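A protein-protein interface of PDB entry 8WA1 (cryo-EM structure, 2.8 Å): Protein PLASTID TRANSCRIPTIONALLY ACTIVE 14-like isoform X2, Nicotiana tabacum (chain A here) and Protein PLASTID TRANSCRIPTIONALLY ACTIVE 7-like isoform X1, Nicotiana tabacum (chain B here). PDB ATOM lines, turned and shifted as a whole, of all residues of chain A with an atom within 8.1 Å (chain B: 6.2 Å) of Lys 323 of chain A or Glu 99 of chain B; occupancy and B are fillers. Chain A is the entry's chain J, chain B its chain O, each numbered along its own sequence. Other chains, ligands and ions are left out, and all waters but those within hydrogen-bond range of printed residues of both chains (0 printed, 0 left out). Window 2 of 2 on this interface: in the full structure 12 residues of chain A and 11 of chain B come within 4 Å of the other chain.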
ATOM      1  N   ARG A 138       0.921 -41.886  19.530  1.00  0.00           N
ATOM      2  CA  ARG A 138       0.470 -41.308  20.786  1.00  0.00           C
ATOM      3  C   ARG A 138      -0.915 -41.839  21.128  1.00  0.00           C
ATOM      4  O   ARG A 138      -1.596 -42.445  20.296  1.00  0.00           O
ATOM      5  CB  ARG A 138       0.452 -39.775  20.725  1.00  0.00           C
ATOM      6  CG  ARG A 138       1.809 -39.135  20.982  1.00  0.00           C
ATOM      7  CD  ARG A 138       1.812 -37.661  20.617  1.00  0.00           C
ATOM      8  NE  ARG A 138       1.890 -37.459  19.174  1.00  0.00           N
ATOM      9  CZ  ARG A 138       3.030 -37.368  18.497  1.00  0.00           C
ATOM     10  NH1 ARG A 138       4.189 -37.461  19.132  1.00  0.00           N
ATOM     11  NH2 ARG A 138       3.011 -37.184  17.183  1.00  0.00           N
ATOM     12  N   ARG A 290      -5.920 -31.376  38.587  1.00  0.00           N
ATOM     13  CA  ARG A 290      -5.542 -29.973  38.695  1.00  0.00           C
ATOM     14  C   ARG A 290      -6.687 -29.118  38.177  1.00  0.00           C
ATOM     15  O   ARG A 290      -7.044 -29.206  36.997  1.00  0.00           O
ATOM     16  CB  ARG A 290      -4.261 -29.678  37.911  1.00  0.00           C
ATOM     17  CG  ARG A 290      -3.964 -28.193  37.771  1.00  0.00           C
ATOM     18  CD  ARG A 290      -2.754 -27.944  36.888  1.00  0.00           C
ATOM     19  NE  ARG A 290      -2.569 -26.520  36.623  1.00  0.00           N
ATOM     20  CZ  ARG A 290      -1.614 -26.023  35.845  1.00  0.00           C
ATOM     21  NH1 ARG A 290      -0.753 -26.835  35.249  1.00  0.00           N
ATOM     22  NH2 ARG A 290      -1.522 -24.714  35.659  1.00  0.00           N
ATOM     23  N   ILE A 291      -7.257 -28.298  39.054  1.00  0.00           N
ATOM     24  CA  ILE A 291      -8.316 -27.363  38.695  1.00  0.00           C
ATOM     25  C   ILE A 291      -7.823 -25.960  39.014  1.00  0.00           C
ATOM     26  O   ILE A 291      -7.503 -25.656  40.172  1.00  0.00           O
ATOM     27  CB  ILE A 291      -9.629 -27.675  39.430  1.00  0.00           C
ATOM     28  CG1 ILE A 291     -10.579 -26.476  39.370  1.00  0.00           C
ATOM     29  CG2 ILE A 291      -9.357 -28.097  40.865  1.00  0.00           C
ATOM     30  CD1 ILE A 291     -11.899 -26.709  40.074  1.00  0.00           C
ATOM     31  N   GLY A 292      -7.757 -25.111  37.995  1.00  0.00           N
ATOM     32  CA  GLY A 292      -7.225 -23.775  38.200  1.00  0.00           C
ATOM     33  C   GLY A 292      -5.750 -23.834  38.542  1.00  0.00           C
ATOM     34  O   GLY A 292      -4.930 -24.357  37.778  1.00  0.00           O
ATOM     35  N   TRP A 320      -5.886 -37.154  32.988  1.00  0.00           N
ATOM     36  CA  TRP A 320      -6.635 -35.970  33.388  1.00  0.00           C
ATOM     37  C   TRP A 320      -6.239 -34.784  32.517  1.00  0.00           C
ATOM     38  O   TRP A 320      -5.053 -34.583  32.237  1.00  0.00           O
ATOM     39  CB  TRP A 320      -6.394 -35.643  34.864  1.00  0.00           C
ATOM     40  CG  TRP A 320      -7.039 -34.366  35.313  1.00  0.00           C
ATOM     41  CD1 TRP A 320      -6.445 -33.143  35.421  1.00  0.00           C
ATOM     42  CD2 TRP A 320      -8.402 -34.186  35.713  1.00  0.00           C
ATOM     43  NE1 TRP A 320      -7.354 -32.212  35.865  1.00  0.00           N
ATOM     44  CE2 TRP A 320      -8.563 -32.828  36.051  1.00  0.00           C
ATOM     45  CE3 TRP A 320      -9.502 -35.042  35.818  1.00  0.00           C
ATOM     46  CZ2 TRP A 320      -9.779 -32.307  36.487  1.00  0.00           C
ATOM     47  CZ3 TRP A 320     -10.709 -34.522  36.250  1.00  0.00           C
ATOM     48  CH2 TRP A 320     -10.837 -33.168  36.580  1.00  0.00           C
ATOM     49  N   ARG A 321      -7.233 -34.007  32.097  1.00  0.00           N
ATOM     50  CA  ARG A 321      -7.025 -32.785  31.330  1.00  0.00           C
ATOM     51  C   ARG A 321      -7.451 -31.601  32.188  1.00  0.00           C
ATOM     52  O   ARG A 321      -8.622 -31.498  32.571  1.00  0.00           O
ATOM     53  CB  ARG A 321      -7.814 -32.817  30.021  1.00  0.00           C
ATOM     54  CG  ARG A 321      -7.534 -31.647  29.094  1.00  0.00           C
ATOM     55  CD  ARG A 321      -8.497 -31.642  27.920  1.00  0.00           C
ATOM     56  NE  ARG A 321      -8.522 -32.926  27.226  1.00  0.00           N
ATOM     57  CZ  ARG A 321      -9.311 -33.202  26.193  1.00  0.00           C
ATOM     58  NH1 ARG A 321     -10.146 -32.282  25.731  1.00  0.00           N
ATOM     59  NH2 ARG A 321      -9.266 -34.397  25.622  1.00  0.00           N
ATOM     60  N   PHE A 322      -6.504 -30.709  32.487  1.00  0.00           N
ATOM     61  CA  PHE A 322      -6.791 -29.618  33.414  1.00  0.00           C
ATOM     62  C   PHE A 322      -7.416 -28.423  32.704  1.00  0.00           C
ATOM     63  O   PHE A 322      -8.215 -27.693  33.302  1.00  0.00           O
ATOM     64  CB  PHE A 322      -5.513 -29.203  34.148  1.00  0.00           C
ATOM     65  CG  PHE A 322      -4.487 -28.549  33.268  1.00  0.00           C
ATOM     66  CD1 PHE A 322      -3.641 -29.312  32.483  1.00  0.00           C
ATOM     67  CD2 PHE A 322      -4.364 -27.170  33.232  1.00  0.00           C
ATOM     68  CE1 PHE A 322      -2.695 -28.716  31.674  1.00  0.00           C
ATOM     69  CE2 PHE A 322      -3.419 -26.565  32.424  1.00  0.00           C
ATOM     70  CZ  PHE A 322      -2.584 -27.339  31.643  1.00  0.00           C
ATOM     71  N   LYS A 323      -7.064 -28.198  31.434  1.00  0.00           N
ATOM     72  CA  LYS A 323      -7.582 -27.030  30.726  1.00  0.00           C
ATOM     73  C   LYS A 323      -9.088 -27.125  30.517  1.00  0.00           C
ATOM     74  O   LYS A 323      -9.823 -26.180  30.827  1.00  0.00           O
ATOM     75  CB  LYS A 323      -6.866 -26.859  29.388  1.00  0.00           C
ATOM     76  CG  LYS A 323      -5.506 -26.189  29.495  1.00  0.00           C
ATOM     77  CD  LYS A 323      -4.961 -25.830  28.123  1.00  0.00           C
ATOM     78  CE  LYS A 323      -3.652 -25.065  28.236  1.00  0.00           C
ATOM     79  NZ  LYS A 323      -3.803 -23.814  29.031  1.00  0.00           N
ATOM     80  N   ASP A 324      -9.569 -28.252  30.000  1.00  0.00           N
ATOM     81  CA  ASP A 324     -10.997 -28.464  29.818  1.00  0.00           C
ATOM     82  C   ASP A 324     -11.673 -29.007  31.068  1.00  0.00           C
ATOM     83  O   ASP A 324     -12.902 -29.131  31.082  1.00  0.00           O
ATOM     84  CB  ASP A 324     -11.252 -29.415  28.645  1.00  0.00           C
ATOM     85  CG  ASP A 324     -11.074 -28.741  27.300  1.00  0.00           C
ATOM     86  OD1 ASP A 324     -10.796 -27.524  27.279  1.00  0.00           O
ATOM     87  OD2 ASP A 324     -11.214 -29.427  26.266  1.00  0.00           O
ATOM     88  N   ARG A 325     -10.903 -29.324  32.107  1.00  0.00           N
ATOM     89  CA  ARG A 325     -11.427 -29.844  33.368  1.00  0.00           C
ATOM     90  C   ARG A 325     -12.279 -31.090  33.124  1.00  0.00           C
ATOM     91  O   ARG A 325     -13.419 -31.204  33.576  1.00  0.00           O
ATOM     92  CB  ARG A 325     -12.213 -28.764  34.114  1.00  0.00           C
ATOM     93  CG  ARG A 325     -11.446 -27.462  34.283  1.00  0.00           C
ATOM     94  CD  ARG A 325     -11.155 -27.169  35.745  1.00  0.00           C
ATOM     95  NE  ARG A 325     -12.339 -26.691  36.453  1.00  0.00           N
ATOM     96  CZ  ARG A 325     -12.635 -25.407  36.628  1.00  0.00           C
ATOM     97  NH1 ARG A 325     -11.831 -24.469  36.147  1.00  0.00           N
ATOM     98  NH2 ARG A 325     -13.733 -25.061  37.283  1.00  0.00           N
ATOM     99  N   MET A 326     -11.696 -32.031  32.384  1.00  0.00           N
ATOM    100  CA  MET A 326     -12.356 -33.279  32.038  1.00  0.00           C
ATOM    101  C   MET A 326     -11.409 -34.447  32.268  1.00  0.00           C
ATOM    102  O   MET A 326     -10.190 -34.317  32.130  1.00  0.00           O
ATOM    103  CB  MET A 326     -12.828 -33.289  30.576  1.00  0.00           C
ATOM    104  CG  MET A 326     -13.804 -32.185  30.215  1.00  0.00           C
ATOM    105  SD  MET A 326     -14.527 -32.418  28.580  1.00  0.00           S
ATOM    106  CE  MET A 326     -13.051 -32.545  27.573  1.00  0.00           C
ATOM    107  N   LEU B  95      -5.252 -29.140  20.038  1.00  0.00           N
ATOM    108  CA  LEU B  95      -3.921 -29.610  20.398  1.00  0.00           C
ATOM    109  C   LEU B  95      -3.271 -28.771  21.487  1.00  0.00           C
ATOM    110  O   LEU B  95      -2.362 -29.265  22.164  1.00  0.00           O
ATOM    111  CB  LEU B  95      -3.017 -29.634  19.163  1.00  0.00           C
ATOM    112  CG  LEU B  95      -3.364 -30.647  18.072  1.00  0.00           C
ATOM    113  CD1 LEU B  95      -2.340 -30.594  16.948  1.00  0.00           C
ATOM    114  CD2 LEU B  95      -3.456 -32.050  18.651  1.00  0.00           C
ATOM    115  N   LEU B  96      -3.706 -27.528  21.675  1.00  0.00           N
ATOM    116  CA  LEU B  96      -3.239 -26.704  22.779  1.00  0.00           C
ATOM    117  C   LEU B  96      -4.030 -26.939  24.057  1.00  0.00           C
ATOM    118  O   LEU B  96      -3.560 -26.569  25.138  1.00  0.00           O
ATOM    119  CB  LEU B  96      -3.298 -25.222  22.400  1.00  0.00           C
ATOM    120  CG  LEU B  96      -2.231 -24.723  21.425  1.00  0.00           C
ATOM    121  CD1 LEU B  96      -2.439 -23.252  21.127  1.00  0.00           C
ATOM    122  CD2 LEU B  96      -0.839 -24.965  21.986  1.00  0.00           C
ATOM    123  N   LEU B  97      -5.212 -27.541  23.961  1.00  0.00           N
ATOM    124  CA  LEU B  97      -5.962 -27.956  25.140  1.00  0.00           C
ATOM    125  C   LEU B  97      -5.388 -29.207  25.793  1.00  0.00           C
ATOM    126  O   LEU B  97      -5.920 -29.656  26.813  1.00  0.00           O
ATOM    127  CB  LEU B  97      -7.432 -28.197  24.779  1.00  0.00           C
ATOM    128  CG  LEU B  97      -8.300 -26.962  24.527  1.00  0.00           C
ATOM    129  CD1 LEU B  97      -9.715 -27.377  24.158  1.00  0.00           C
ATOM    130  CD2 LEU B  97      -8.304 -26.046  25.741  1.00  0.00           C
ATOM    131  N   ASN B  98      -4.320 -29.778  25.233  1.00  0.00           N
ATOM    132  CA  ASN B  98      -3.664 -30.957  25.786  1.00  0.00           C
ATOM    133  C   ASN B  98      -2.188 -30.693  26.064  1.00  0.00           C
ATOM    134  O   ASN B  98      -1.365 -31.608  26.010  1.00  0.00           O
ATOM    135  CB  ASN B  98      -3.820 -32.154  24.848  1.00  0.00           C
ATOM    136  CG  ASN B  98      -5.268 -32.506  24.590  1.00  0.00           C
ATOM    137  OD1 ASN B  98      -5.725 -32.504  23.447  1.00  0.00           O
ATOM    138  ND2 ASN B  98      -6.001 -32.813  25.653  1.00  0.00           N
ATOM    139  N   GLU B  99      -1.840 -29.444  26.363  1.00  0.00           N
ATOM    140  CA  GLU B  99      -0.450 -29.062  26.564  1.00  0.00           C
ATOM    141  C   GLU B  99      -0.383 -28.008  27.656  1.00  0.00           C
ATOM    142  O   GLU B  99      -1.174 -27.060  27.653  1.00  0.00           O
ATOM    143  CB  GLU B  99       0.166 -28.527  25.267  1.00  0.00           C
ATOM    144  CG  GLU B  99       1.684 -28.509  25.249  1.00  0.00           C
ATOM    145  CD  GLU B  99       2.283 -29.901  25.190  1.00  0.00           C
ATOM    146  OE1 GLU B  99       3.252 -30.165  25.932  1.00  0.00           O
ATOM    147  OE2 GLU B  99       1.783 -30.733  24.404  1.00  0.00           O
ATOM    148  N   ASP B 100       0.559 -28.174  28.585  1.00  0.00           N
ATOM    149  CA  ASP B 100       0.708 -27.201  29.662  1.00  0.00           C
ATOM    150  C   ASP B 100       1.320 -25.904  29.150  1.00  0.00           C
ATOM    151  O   ASP B 100       0.740 -24.825  29.314  1.00  0.00           O
ATOM    152  CB  ASP B 100       1.555 -27.790  30.789  1.00  0.00           C
ATOM    153  CG  ASP B 100       1.738 -26.825  31.945  1.00  0.00           C
ATOM    154  OD1 ASP B 100       0.742 -26.534  32.640  1.00  0.00           O
ATOM    155  OD2 ASP B 100       2.875 -26.357  32.157  1.00  0.00           O
ATOM    156  N   ASN B 101       2.486 -25.990  28.514  1.00  0.00           N
ATOM    157  CA  ASN B 101       3.200 -24.824  28.010  1.00  0.00           C
ATOM    158  C   ASN B 101       3.121 -24.818  26.491  1.00  0.00           C
ATOM    159  O   ASN B 101       3.522 -25.789  25.841  1.00  0.00           O
ATOM    160  CB  ASN B 101       4.657 -24.830  28.475  1.00  0.00           C
ATOM    161  CG  ASN B 101       5.376 -23.536  28.154  1.00  0.00           C
ATOM    162  OD1 ASN B 101       4.745 -22.509  27.904  1.00  0.00           O
ATOM    163  ND2 ASN B 101       6.703 -23.577  28.161  1.00  0.00           N
ATOM    164  N   ARG B 102       2.602 -23.723  25.928  1.00  0.00           N
ATOM    165  CA  ARG B 102       2.454 -23.635  24.479  1.00  0.00           C
ATOM    166  C   ARG B 102       3.796 -23.454  23.782  1.00  0.00           C
ATOM    167  O   ARG B 102       3.937 -23.814  22.608  1.00  0.00           O
ATOM    168  CB  ARG B 102       1.503 -22.492  24.120  1.00  0.00           C
ATOM    169  CG  ARG B 102       1.892 -21.140  24.698  1.00  0.00           C
ATOM    170  CD  ARG B 102       0.809 -20.104  24.437  1.00  0.00           C
ATOM    171  NE  ARG B 102       1.211 -18.767  24.861  1.00  0.00           N
ATOM    172  CZ  ARG B 102       1.004 -18.273  26.078  1.00  0.00           C
ATOM    173  NH1 ARG B 102       0.396 -19.007  26.999  1.00  0.00           N
ATOM    174  NH2 ARG B 102       1.404 -17.043  26.373  1.00  0.00           N
ATOM    175  N   ASP B 104       6.736 -24.944  24.503  1.00  0.00           N
ATOM    176  CA  ASP B 104       7.310 -26.262  24.254  1.00  0.00           C
ATOM    177  C   ASP B 104       6.579 -26.981  23.130  1.00  0.00           C
ATOM    178  O   ASP B 104       7.206 -27.701  22.346  1.00  0.00           O
ATOM    179  CB  ASP B 104       7.280 -27.097  25.532  1.00  0.00           C
ATOM    180  CG  ASP B 104       8.040 -26.445  26.668  1.00  0.00           C
ATOM    181  OD1 ASP B 104       8.598 -25.348  26.456  1.00  0.00           O
ATOM    182  OD2 ASP B 104       8.080 -27.028  27.773  1.00  0.00           O
ATOM    183  N   PHE B 105       5.263 -26.790  23.029  1.00  0.00           N
ATOM    184  CA  PHE B 105       4.510 -27.366  21.920  1.00  0.00           C
ATOM    185  C   PHE B 105       4.958 -26.775  20.590  1.00  0.00           C
ATOM    186  O   PHE B 105       5.113 -27.499  19.598  1.00  0.00           O
ATOM    187  CB  PHE B 105       3.015 -27.141  22.142  1.00  0.00           C
ATOM    188  CG  PHE B 105       2.132 -27.944  21.232  1.00  0.00           C
ATOM    189  CD1 PHE B 105       2.159 -29.328  21.262  1.00  0.00           C
ATOM    190  CD2 PHE B 105       1.256 -27.315  20.364  1.00  0.00           C
ATOM    191  CE1 PHE B 105       1.341 -30.069  20.432  1.00  0.00           C
ATOM    192  CE2 PHE B 105       0.433 -28.050  19.535  1.00  0.00           C
ATOM    193  CZ  PHE B 105       0.478 -29.429  19.566  1.00  0.00           C
ATOM    194  N   GLU B 108       8.311 -28.284  19.748  1.00  0.00           N
ATOM    195  CA  GLU B 108       8.170 -29.671  19.315  1.00  0.00           C
ATOM    196  C   GLU B 108       7.648 -29.749  17.886  1.00  0.00           C
ATOM    197  O   GLU B 108       8.136 -30.546  17.075  1.00  0.00           O
ATOM    198  CB  GLU B 108       7.244 -30.420  20.272  1.00  0.00           C
ATOM    199  CG  GLU B 108       7.028 -31.879  19.920  1.00  0.00           C
ATOM    200  CD  GLU B 108       6.127 -32.586  20.911  1.00  0.00           C
ATOM    201  OE1 GLU B 108       5.531 -31.902  21.769  1.00  0.00           O
ATOM    202  OE2 GLU B 108       6.017 -33.827  20.836  1.00  0.00           O
ATOM    203  N   ARG B 137      -1.004 -35.486  13.328  1.00  0.00           N
ATOM    204  CA  ARG B 137      -1.386 -35.528  14.737  1.00  0.00           C
ATOM    205  C   ARG B 137      -2.901 -35.587  14.897  1.00  0.00           C
ATOM    206  O   ARG B 137      -3.414 -36.221  15.827  1.00  0.00           O
ATOM    207  CB  ARG B 137      -0.805 -34.324  15.477  1.00  0.00           C
ATOM    208  CG  ARG B 137       0.706 -34.370  15.620  1.00  0.00           C
ATOM    209  CD  ARG B 137       1.171 -33.637  16.866  1.00  0.00           C
ATOM    210  NE  ARG B 137       2.616 -33.746  17.050  1.00  0.00           N
ATOM    211  CZ  ARG B 137       3.262 -33.349  18.139  1.00  0.00           C
ATOM    212  NH1 ARG B 137       2.593 -32.815  19.152  1.00  0.00           N
ATOM    213  NH2 ARG B 137       4.578 -33.487  18.218  1.00  0.00           N
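The guanidinium group (NH2) of Arg 138 of chain A sits close to the guanidinium group (NE) of Arg 137 of chain B, 3.5 Å away.
The guanidinium group (NH1) of Arg 290 of chain A is in salt-bridge range of the side-chain carboxylate (OD1) of Asp 100 of chain B (3.0 Å).
The side-chain amide nitrogen of Asn 98 of chain B lies close to the guanidinium group of Arg 321 of chain A.
N of Arg 321 of chain A lies within hydrogen-bond range of O of Met 326 of chain A.
The backbone carbonyl oxygen of Gly 292 of chain A sits at hydrogen-bond distance from the guanidinium group of Arg 290 of chain A, 3.4 Å away.
NH2 of Arg 137 of chain B lies within salt-bridge range of OE2 of Glu 108 of chain B (3.0 Å).
The backbone carbonyl oxygen (O) of Arg 290 of chain A sits at hydrogen-bond distance from the indole nitrogen (NE1) of Trp 320 of chain A (3.2 Å).
The guanidinium group (NH1) of Arg 321 of chain A lies within salt-bridge range of the side-chain carboxylate (OD2) of Asp 324 of chain A (3.1 Å).
O of Leu 97 of chain B touches CG of Arg 321 of chain A (3.4 Å).
Phe 322 of chain A touches Asp 100 of chain B.
CD of Lys 323 of chain A touches O of Leu 96 of chain B, 3.4 Å away.
CA of Leu 97 of chain B touches CD of Lys 323 of chain A, at 3.8 Å.
Glu 99 of chain B touches Lys 323 of chain A (O to CE, 3.2 Å).
Asp 324 of chain A touches Leu 97 of chain B.
Of the printed residues of chain B, Arg 138 of chain A touches Arg 137.
Of the printed residues of chain B, Phe 322 of chain A touches Asp 100.
Lys 323 of chain A touches three residues of chain B.
Printed residues of chain B within 4 Å of Asp 324 of chain A: Leu 97 (3.3 Å).
Of the printed residues of chain A, Glu 99 of chain B touches Lys 323 (3.2 Å).
Asn 101 of chain B touches none of the printed residues of chain A.
Of the printed residues of chain A, Arg 137 of chain B touches Arg 138 (3.5 Å).
Of the 12 printed residues of chain B, 6 touch a printed residue of chain A.
Among the printed residues, Asp or Glu carboxylates within 4 Å of a Lys or Arg side-chain nitrogen of the other chain: Arg 290 of chain A with Asp 100 of chain B.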
